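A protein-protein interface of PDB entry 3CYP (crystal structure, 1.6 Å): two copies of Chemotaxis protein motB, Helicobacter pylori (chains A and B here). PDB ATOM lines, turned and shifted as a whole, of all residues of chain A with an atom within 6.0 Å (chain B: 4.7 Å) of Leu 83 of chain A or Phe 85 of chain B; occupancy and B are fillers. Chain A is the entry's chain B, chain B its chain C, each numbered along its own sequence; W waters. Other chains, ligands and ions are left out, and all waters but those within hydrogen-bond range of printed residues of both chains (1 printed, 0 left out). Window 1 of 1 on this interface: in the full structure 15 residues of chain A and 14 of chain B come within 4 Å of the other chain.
A ring nitrogen (ND1) of His 38 of chain A lies close to the backbone carbonyl oxygen (O) of Asn 81 of chain A (3.3 Å). The side-chain amide oxygen of Asn 79 of chain A sits at hydrogen-bond distance from the backbone NH of Asn 81 of chain A, at 2.9 Å. The side-chain hydroxyl (OG) of Ser 87 of chain B sits at hydrogen-bond distance from the backbone NH (N) of Ala 63 of chain B, 3.4 Å away.
Among the printed residues, merely in contact across the chains: Met 70 of chain A with Tyr 67 of chain B, Met 70 of chain A with Phe 85 of chain B, Ile 74 of chain A with Tyr 67 of chain B, Pro 80 of chain A with Ala 63 of chain B, Pro 80 of chain A with Phe 85 of chain B, Asn 81 of chain A with Ala 63 of chain B, Asn 81 of chain A with Ser 87 of chain B, Leu 83 of chain A with Phe 85 of chain B and Phe 85 of chain A with Met 70 of chain B.
Of the printed residues of chain B, Leu 83 of chain A touches Phe 85. Phe 85 of chain B touches just these residues of chain A: Met 70 (3.7 Å), Pro 80 (3.4 Å) and Leu 83 (3.4 Å). Printed residues of chain B within 4 Å of Pro 80 of chain A: Ala 63 (3.98 Å) and Phe 85 (3.4 Å). Of the printed residues of chain B, Phe 85 of chain A touches Met 70. Printed residues of chain A within 4 Å of Ser 87 of chain B: Asn 81. Asn 79 of chain A touches none of the printed residues of chain B.
Of the 16 printed residues of chain A, 6 touch a printed residue of chain B. Hydrophobic or aromatic side chains of chain A within 4 Å of the printed part of chain B: Met 70, Ile 74 and Phe 85.
Met 70 of chain A touches Phe 85 of chain B, and with the chains exchanged Phe 85 of chain A touches Met 70 of chain B.
Water W1 bridges the backbone carbonyl oxygen (O) of Phe 85 of chain B (2.6 Å) and the backbone carbonyl oxygen (O) of Leu 83 of chain A (2.8 Å).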
ATOM      1  N   ILE A  30      -4.303 -30.512 -27.546  1.00  0.00           N
ATOM      2  CA  ILE A  30      -5.230 -29.617 -28.244  1.00  0.00           C
ATOM      3  C   ILE A  30      -4.887 -28.147 -28.026  1.00  0.00           C
ATOM      4  O   ILE A  30      -4.994 -27.356 -28.959  1.00  0.00           O
ATOM      5  CB  ILE A  30      -6.699 -29.924 -27.874  1.00  0.00           C
ATOM      6  CG1 ILE A  30      -7.107 -31.264 -28.500  1.00  0.00           C
ATOM      7  CG2 ILE A  30      -7.594 -28.799 -28.324  1.00  0.00           C
ATOM      8  CD1 ILE A  30      -8.487 -31.809 -27.967  1.00  0.00           C
ATOM      9  N   HIS A  38     -10.825 -26.449 -34.807  1.00  0.00           N
ATOM     10  CA  HIS A  38     -11.898 -26.904 -33.889  1.00  0.00           C
ATOM     11  C   HIS A  38     -11.908 -28.428 -33.793  1.00  0.00           C
ATOM     12  O   HIS A  38     -11.357 -29.108 -34.678  1.00  0.00           O
ATOM     13  CB  HIS A  38     -13.231 -26.356 -34.318  1.00  0.00           C
ATOM     14  CG  HIS A  38     -13.361 -24.887 -34.075  1.00  0.00           C
ATOM     15  ND1 HIS A  38     -14.519 -24.314 -33.611  1.00  0.00           N
ATOM     16  CD2 HIS A  38     -12.463 -23.881 -34.186  1.00  0.00           C
ATOM     17  CE1 HIS A  38     -14.340 -23.012 -33.463  1.00  0.00           C
ATOM     18  NE2 HIS A  38     -13.100 -22.718 -33.809  1.00  0.00           N
ATOM     19  N   ILE A  39     -12.495 -28.933 -32.703  1.00  0.00           N
ATOM     20  CA  ILE A  39     -12.462 -30.339 -32.310  1.00  0.00           C
ATOM     21  C   ILE A  39     -13.903 -30.782 -32.110  1.00  0.00           C
ATOM     22  O   ILE A  39     -14.632 -30.126 -31.360  1.00  0.00           O
ATOM     23  CB  ILE A  39     -11.731 -30.490 -30.962  1.00  0.00           C
ATOM     24  CG1 ILE A  39     -10.283 -29.977 -31.045  1.00  0.00           C
ATOM     25  CG2 ILE A  39     -11.852 -31.888 -30.432  1.00  0.00           C
ATOM     26  CD1 ILE A  39      -9.417 -30.738 -31.940  1.00  0.00           C
ATOM     27  N   ASN A  40     -14.320 -31.833 -32.809  1.00  0.00           N
ATOM     28  CA  ASN A  40     -15.658 -32.410 -32.654  1.00  0.00           C
ATOM     29  C   ASN A  40     -15.490 -33.760 -31.971  1.00  0.00           C
ATOM     30  O   ASN A  40     -14.726 -34.609 -32.464  1.00  0.00           O
ATOM     31  CB  ASN A  40     -16.297 -32.617 -34.006  1.00  0.00           C
ATOM     32  CG  ASN A  40     -17.666 -33.233 -33.943  1.00  0.00           C
ATOM     33  OD1 ASN A  40     -17.946 -34.217 -34.641  1.00  0.00           O
ATOM     34  ND2 ASN A  40     -18.563 -32.583 -33.236  1.00  0.00           N
ATOM     35  N   VAL A  41     -16.141 -33.913 -30.820  1.00  0.00           N
ATOM     36  CA  VAL A  41     -16.028 -35.099 -29.967  1.00  0.00           C
ATOM     37  C   VAL A  41     -17.211 -35.973 -30.325  1.00  0.00           C
ATOM     38  O   VAL A  41     -18.355 -35.607 -30.066  1.00  0.00           O
ATOM     39  CB  VAL A  41     -16.062 -34.713 -28.432  1.00  0.00           C
ATOM     40  CG1 VAL A  41     -15.923 -35.955 -27.561  1.00  0.00           C
ATOM     41  CG2 VAL A  41     -14.988 -33.677 -28.104  1.00  0.00           C
ATOM     42  N   MET A  70     -16.060 -34.307 -23.722  1.00  0.00           N
ATOM     43  CA  MET A  70     -15.931 -32.887 -24.019  1.00  0.00           C
ATOM     44  C   MET A  70     -15.768 -32.079 -22.730  1.00  0.00           C
ATOM     45  O   MET A  70     -14.981 -31.159 -22.691  1.00  0.00           O
ATOM     46  CB  MET A  70     -17.140 -32.373 -24.788  1.00  0.00           C
ATOM     47  CG  MET A  70     -16.946 -30.941 -25.333  1.00  0.00           C
ATOM     48  SD  MET A  70     -18.372 -30.303 -26.169  1.00  0.00           S
ATOM     49  CE  MET A  70     -19.495 -30.026 -24.758  1.00  0.00           C
ATOM     50  N   LEU A  73     -12.308 -32.533 -21.437  1.00  0.00           N
ATOM     51  CA  LEU A  73     -11.367 -31.699 -22.184  1.00  0.00           C
ATOM     52  C   LEU A  73     -11.393 -30.231 -21.728  1.00  0.00           C
ATOM     53  O   LEU A  73     -10.346 -29.570 -21.647  1.00  0.00           O
ATOM     54  CB  LEU A  73     -11.657 -31.810 -23.694  1.00  0.00           C
ATOM     55  CG  LEU A  73     -11.351 -33.146 -24.338  1.00  0.00           C
ATOM     56  CD1 LEU A  73     -11.956 -33.106 -25.787  1.00  0.00           C
ATOM     57  CD2 LEU A  73      -9.823 -33.341 -24.391  1.00  0.00           C
ATOM     58  N   ILE A  74     -12.586 -29.698 -21.444  1.00  0.00           N
ATOM     59  CA  ILE A  74     -12.737 -28.318 -21.019  1.00  0.00           C
ATOM     60  C   ILE A  74     -12.177 -28.124 -19.601  1.00  0.00           C
ATOM     61  O   ILE A  74     -11.477 -27.143 -19.345  1.00  0.00           O
ATOM     62  CB  ILE A  74     -14.213 -27.864 -21.113  1.00  0.00           C
ATOM     63  CG1 ILE A  74     -14.631 -27.726 -22.590  1.00  0.00           C
ATOM     64  CG2 ILE A  74     -14.430 -26.578 -20.392  1.00  0.00           C
ATOM     65  CD1 ILE A  74     -16.181 -27.688 -22.808  1.00  0.00           C
ATOM     66  N   VAL A  78      -9.100 -27.042 -22.498  1.00  0.00           N
ATOM     67  CA  VAL A  78      -9.454 -26.755 -23.886  1.00  0.00           C
ATOM     68  C   VAL A  78     -10.521 -25.659 -23.916  1.00  0.00           C
ATOM     69  O   VAL A  78     -11.481 -25.684 -23.129  1.00  0.00           O
ATOM     70  CB  VAL A  78      -9.940 -28.008 -24.643  1.00  0.00           C
ATOM     71  CG1 VAL A  78     -10.420 -27.623 -26.082  1.00  0.00           C
ATOM     72  CG2 VAL A  78      -8.835 -29.052 -24.719  1.00  0.00           C
ATOM     73  N   ASN A  79     -10.371 -24.697 -24.806  1.00  0.00           N
ATOM     74  CA  ASN A  79     -11.344 -23.635 -24.921  1.00  0.00           C
ATOM     75  C   ASN A  79     -12.696 -24.139 -25.434  1.00  0.00           C
ATOM     76  O   ASN A  79     -12.742 -24.734 -26.483  1.00  0.00           O
ATOM     77  CB  ASN A  79     -10.863 -22.552 -25.878  1.00  0.00           C
ATOM     78  CG  ASN A  79     -11.575 -21.258 -25.628  1.00  0.00           C
ATOM     79  OD1 ASN A  79     -12.677 -21.012 -26.148  1.00  0.00           O
ATOM     80  ND2 ASN A  79     -10.960 -20.412 -24.801  1.00  0.00           N
ATOM     81  N   PRO A  80     -13.806 -23.886 -24.715  1.00  0.00           N
ATOM     82  CA  PRO A  80     -15.111 -24.321 -25.256  1.00  0.00           C
ATOM     83  C   PRO A  80     -15.400 -23.857 -26.691  1.00  0.00           C
ATOM     84  O   PRO A  80     -16.094 -24.538 -27.451  1.00  0.00           O
ATOM     85  CB  PRO A  80     -16.123 -23.723 -24.249  1.00  0.00           C
ATOM     86  CG  PRO A  80     -15.381 -23.504 -23.028  1.00  0.00           C
ATOM     87  CD  PRO A  80     -13.949 -23.235 -23.396  1.00  0.00           C
ATOM     88  N   ASN A  81     -14.863 -22.696 -27.094  1.00  0.00           N
ATOM     89  CA  ASN A  81     -15.113 -22.214 -28.438  1.00  0.00           C
ATOM     90  C   ASN A  81     -14.608 -23.183 -29.498  1.00  0.00           C
ATOM     91  O   ASN A  81     -15.192 -23.238 -30.588  1.00  0.00           O
ATOM     92  CB  ASN A  81     -14.497 -20.838 -28.690  1.00  0.00           C
ATOM     93  CG  ASN A  81     -14.956 -20.242 -30.011  1.00  0.00           C
ATOM     94  OD1 ASN A  81     -16.149 -20.140 -30.283  1.00  0.00           O
ATOM     95  ND2 ASN A  81     -13.986 -19.918 -30.888  1.00  0.00           N
ATOM     96  N   GLN A  82     -13.560 -23.928 -29.157  1.00  0.00           N
ATOM     97  CA  GLN A  82     -13.020 -24.899 -30.117  1.00  0.00           C
ATOM     98  C   GLN A  82     -13.764 -26.244 -30.145  1.00  0.00           C
ATOM     99  O   GLN A  82     -13.497 -27.105 -30.982  1.00  0.00           O
ATOM    100  CB  GLN A  82     -11.542 -25.118 -29.841  1.00  0.00           C
ATOM    101  CG  GLN A  82     -10.714 -24.003 -30.353  1.00  0.00           C
ATOM    102  CD  GLN A  82      -9.300 -24.104 -29.855  1.00  0.00           C
ATOM    103  OE1 GLN A  82      -9.020 -23.839 -28.672  1.00  0.00           O
ATOM    104  NE2 GLN A  82      -8.391 -24.505 -30.745  1.00  0.00           N
ATOM    105  N   LEU A  83     -14.710 -26.437 -29.243  1.00  0.00           N
ATOM    106  CA  LEU A  83     -15.307 -27.744 -29.050  1.00  0.00           C
ATOM    107  C   LEU A  83     -16.781 -27.870 -29.426  1.00  0.00           C
ATOM    108  O   LEU A  83     -17.559 -26.911 -29.344  1.00  0.00           O
ATOM    109  CB  LEU A  83     -15.151 -28.145 -27.608  1.00  0.00           C
ATOM    110  CG  LEU A  83     -13.791 -28.684 -27.223  1.00  0.00           C
ATOM    111  CD1 LEU A  83     -13.662 -28.683 -25.718  1.00  0.00           C
ATOM    112  CD2 LEU A  83     -13.478 -30.076 -27.785  1.00  0.00           C
ATOM    113  N   SER A  84     -17.141 -29.073 -29.834  1.00  0.00           N
ATOM    114  CA  SER A  84     -18.504 -29.501 -30.011  1.00  0.00           C
ATOM    115  C   SER A  84     -18.564 -30.987 -29.768  1.00  0.00           C
ATOM    116  O   SER A  84     -17.539 -31.639 -29.709  1.00  0.00           O
ATOM    117  CB  SER A  84     -18.991 -29.220 -31.418  1.00  0.00           C
ATOM    118  OG  SER A  84     -18.214 -29.896 -32.383  1.00  0.00           O
ATOM    119  N   PHE A  85     -19.783 -31.510 -29.635  1.00  0.00           N
ATOM    120  CA  PHE A  85     -19.952 -32.967 -29.480  1.00  0.00           C
ATOM    121  C   PHE A  85     -21.118 -33.448 -30.350  1.00  0.00           C
ATOM    122  O   PHE A  85     -22.074 -32.691 -30.643  1.00  0.00           O
ATOM    123  CB  PHE A  85     -20.108 -33.342 -28.006  1.00  0.00           C
ATOM    124  CG  PHE A  85     -21.483 -33.095 -27.455  1.00  0.00           C
ATOM    125  CD1 PHE A  85     -21.872 -31.814 -27.078  1.00  0.00           C
ATOM    126  CD2 PHE A  85     -22.394 -34.112 -27.306  1.00  0.00           C
ATOM    127  CE1 PHE A  85     -23.137 -31.560 -26.545  1.00  0.00           C
ATOM    128  CE2 PHE A  85     -23.665 -33.859 -26.802  1.00  0.00           C
ATOM    129  CZ  PHE A  85     -24.039 -32.564 -26.425  1.00  0.00           C
ATOM    130  N   ASN B  40     -30.412 -25.894 -29.770  1.00  0.00           N
ATOM    131  CA  ASN B  40     -29.057 -25.285 -29.953  1.00  0.00           C
ATOM    132  C   ASN B  40     -29.031 -24.067 -29.057  1.00  0.00           C
ATOM    133  O   ASN B  40     -29.869 -23.177 -29.183  1.00  0.00           O
ATOM    134  CB  ASN B  40     -28.823 -24.918 -31.440  1.00  0.00           C
ATOM    135  CG  ASN B  40     -27.507 -24.287 -31.714  1.00  0.00           C
ATOM    136  OD1 ASN B  40     -27.451 -23.170 -32.264  1.00  0.00           O
ATOM    137  ND2 ASN B  40     -26.468 -24.955 -31.371  1.00  0.00           N
ATOM    138  N   VAL B  41     -28.063 -24.065 -28.132  1.00  0.00           N
ATOM    139  CA  VAL B  41     -27.904 -23.022 -27.143  1.00  0.00           C
ATOM    140  C   VAL B  41     -26.834 -22.095 -27.717  1.00  0.00           C
ATOM    141  O   VAL B  41     -25.645 -22.482 -27.888  1.00  0.00           O
ATOM    142  CB  VAL B  41     -27.414 -23.618 -25.820  1.00  0.00           C
ATOM    143  CG1 VAL B  41     -27.213 -22.512 -24.791  1.00  0.00           C
ATOM    144  CG2 VAL B  41     -28.371 -24.723 -25.356  1.00  0.00           C
ATOM    145  N   ALA B  63     -18.917 -18.483 -26.269  1.00  0.00           N
ATOM    146  CA  ALA B  63     -18.889 -19.959 -26.109  1.00  0.00           C
ATOM    147  C   ALA B  63     -19.068 -20.414 -24.683  1.00  0.00           C
ATOM    148  O   ALA B  63     -19.813 -21.389 -24.402  1.00  0.00           O
ATOM    149  CB  ALA B  63     -17.576 -20.524 -26.644  1.00  0.00           C
ATOM    150  N   ALA B  66     -22.741 -19.936 -23.633  1.00  0.00           N
ATOM    151  CA  ALA B  66     -23.621 -20.955 -24.211  1.00  0.00           C
ATOM    152  C   ALA B  66     -23.353 -22.301 -23.576  1.00  0.00           C
ATOM    153  O   ALA B  66     -24.286 -23.027 -23.209  1.00  0.00           O
ATOM    154  CB  ALA B  66     -23.446 -21.006 -25.696  1.00  0.00           C
ATOM    155  N   TYR B  67     -22.075 -22.671 -23.456  1.00  0.00           N
ATOM    156  CA  TYR B  67     -21.701 -23.944 -22.843  1.00  0.00           C
ATOM    157  C   TYR B  67     -22.252 -24.068 -21.407  1.00  0.00           C
ATOM    158  O   TYR B  67     -22.830 -25.071 -21.020  1.00  0.00           O
ATOM    159  CB  TYR B  67     -20.177 -24.086 -22.883  1.00  0.00           C
ATOM    160  CG  TYR B  67     -19.652 -25.243 -22.060  1.00  0.00           C
ATOM    161  CD1 TYR B  67     -20.003 -26.551 -22.372  1.00  0.00           C
ATOM    162  CD2 TYR B  67     -18.862 -25.032 -20.936  1.00  0.00           C
ATOM    163  CE1 TYR B  67     -19.563 -27.635 -21.596  1.00  0.00           C
ATOM    164  CE2 TYR B  67     -18.392 -26.116 -20.165  1.00  0.00           C
ATOM    165  CZ  TYR B  67     -18.739 -27.411 -20.523  1.00  0.00           C
ATOM    166  OH  TYR B  67     -18.293 -28.521 -19.805  1.00  0.00           O
ATOM    167  N   MET B  70     -25.884 -24.567 -21.387  1.00  0.00           N
ATOM    168  CA  MET B  70     -26.130 -25.971 -21.809  1.00  0.00           C
ATOM    169  C   MET B  70     -25.901 -26.990 -20.659  1.00  0.00           C
ATOM    170  O   MET B  70     -26.705 -27.930 -20.464  1.00  0.00           O
ATOM    171  CB  MET B  70     -25.291 -26.336 -23.038  1.00  0.00           C
ATOM    172  CG  MET B  70     -25.780 -27.599 -23.662  1.00  0.00           C
ATOM    173  SD  MET B  70     -24.632 -28.218 -24.942  1.00  0.00           S
ATOM    174  CE  MET B  70     -23.217 -28.693 -23.951  1.00  0.00           C
ATOM    175  N   SER B  84     -26.898 -29.012 -28.264  1.00  0.00           N
ATOM    176  CA  SER B  84     -25.624 -28.534 -28.773  1.00  0.00           C
ATOM    177  C   SER B  84     -25.489 -27.086 -28.337  1.00  0.00           C
ATOM    178  O   SER B  84     -26.471 -26.472 -27.909  1.00  0.00           O
ATOM    179  CB  SER B  84     -25.593 -28.642 -30.282  1.00  0.00           C
ATOM    180  OG  SER B  84     -26.548 -27.832 -30.892  1.00  0.00           O
ATOM    181  N   PHE B  85     -24.279 -26.552 -28.449  1.00  0.00           N
ATOM    182  CA  PHE B  85     -24.040 -25.118 -28.207  1.00  0.00           C
ATOM    183  C   PHE B  85     -23.226 -24.493 -29.315  1.00  0.00           C
ATOM    184  O   PHE B  85     -22.419 -25.187 -29.990  1.00  0.00           O
ATOM    185  CB  PHE B  85     -23.404 -24.865 -26.845  1.00  0.00           C
ATOM    186  CG  PHE B  85     -21.916 -25.173 -26.770  1.00  0.00           C
ATOM    187  CD1 PHE B  85     -21.469 -26.489 -26.573  1.00  0.00           C
ATOM    188  CD2 PHE B  85     -20.969 -24.157 -26.917  1.00  0.00           C
ATOM    189  CE1 PHE B  85     -20.107 -26.768 -26.480  1.00  0.00           C
ATOM    190  CE2 PHE B  85     -19.600 -24.456 -26.839  1.00  0.00           C
ATOM    191  CZ  PHE B  85     -19.189 -25.765 -26.627  1.00  0.00           C
ATOM    192  N   SER B  86     -23.440 -23.201 -29.519  1.00  0.00           N
ATOM    193  CA  SER B  86     -22.791 -22.502 -30.598  1.00  0.00           C
ATOM    194  C   SER B  86     -22.415 -21.130 -30.150  1.00  0.00           C
ATOM    195  O   SER B  86     -23.178 -20.460 -29.471  1.00  0.00           O
ATOM    196  CB  SER B  86     -23.662 -22.447 -31.836  1.00  0.00           C
ATOM    197  OG  SER B  86     -23.977 -23.736 -32.330  1.00  0.00           O
ATOM    198  N   SER B  87     -21.220 -20.713 -30.523  1.00  0.00           N
ATOM    199  CA  SER B  87     -20.779 -19.347 -30.246  1.00  0.00           C
ATOM    200  C   SER B  87     -20.923 -18.458 -31.465  1.00  0.00           C
ATOM    201  O   SER B  87     -20.394 -18.768 -32.524  1.00  0.00           O
ATOM    202  CB  SER B  87     -19.334 -19.333 -29.763  1.00  0.00           C
ATOM    203  OG  SER B  87     -18.970 -17.953 -29.645  1.00  0.00           O
HETATM  204  O   HOH W   1     -20.343 -26.780 -29.910  1.00  0.00           O
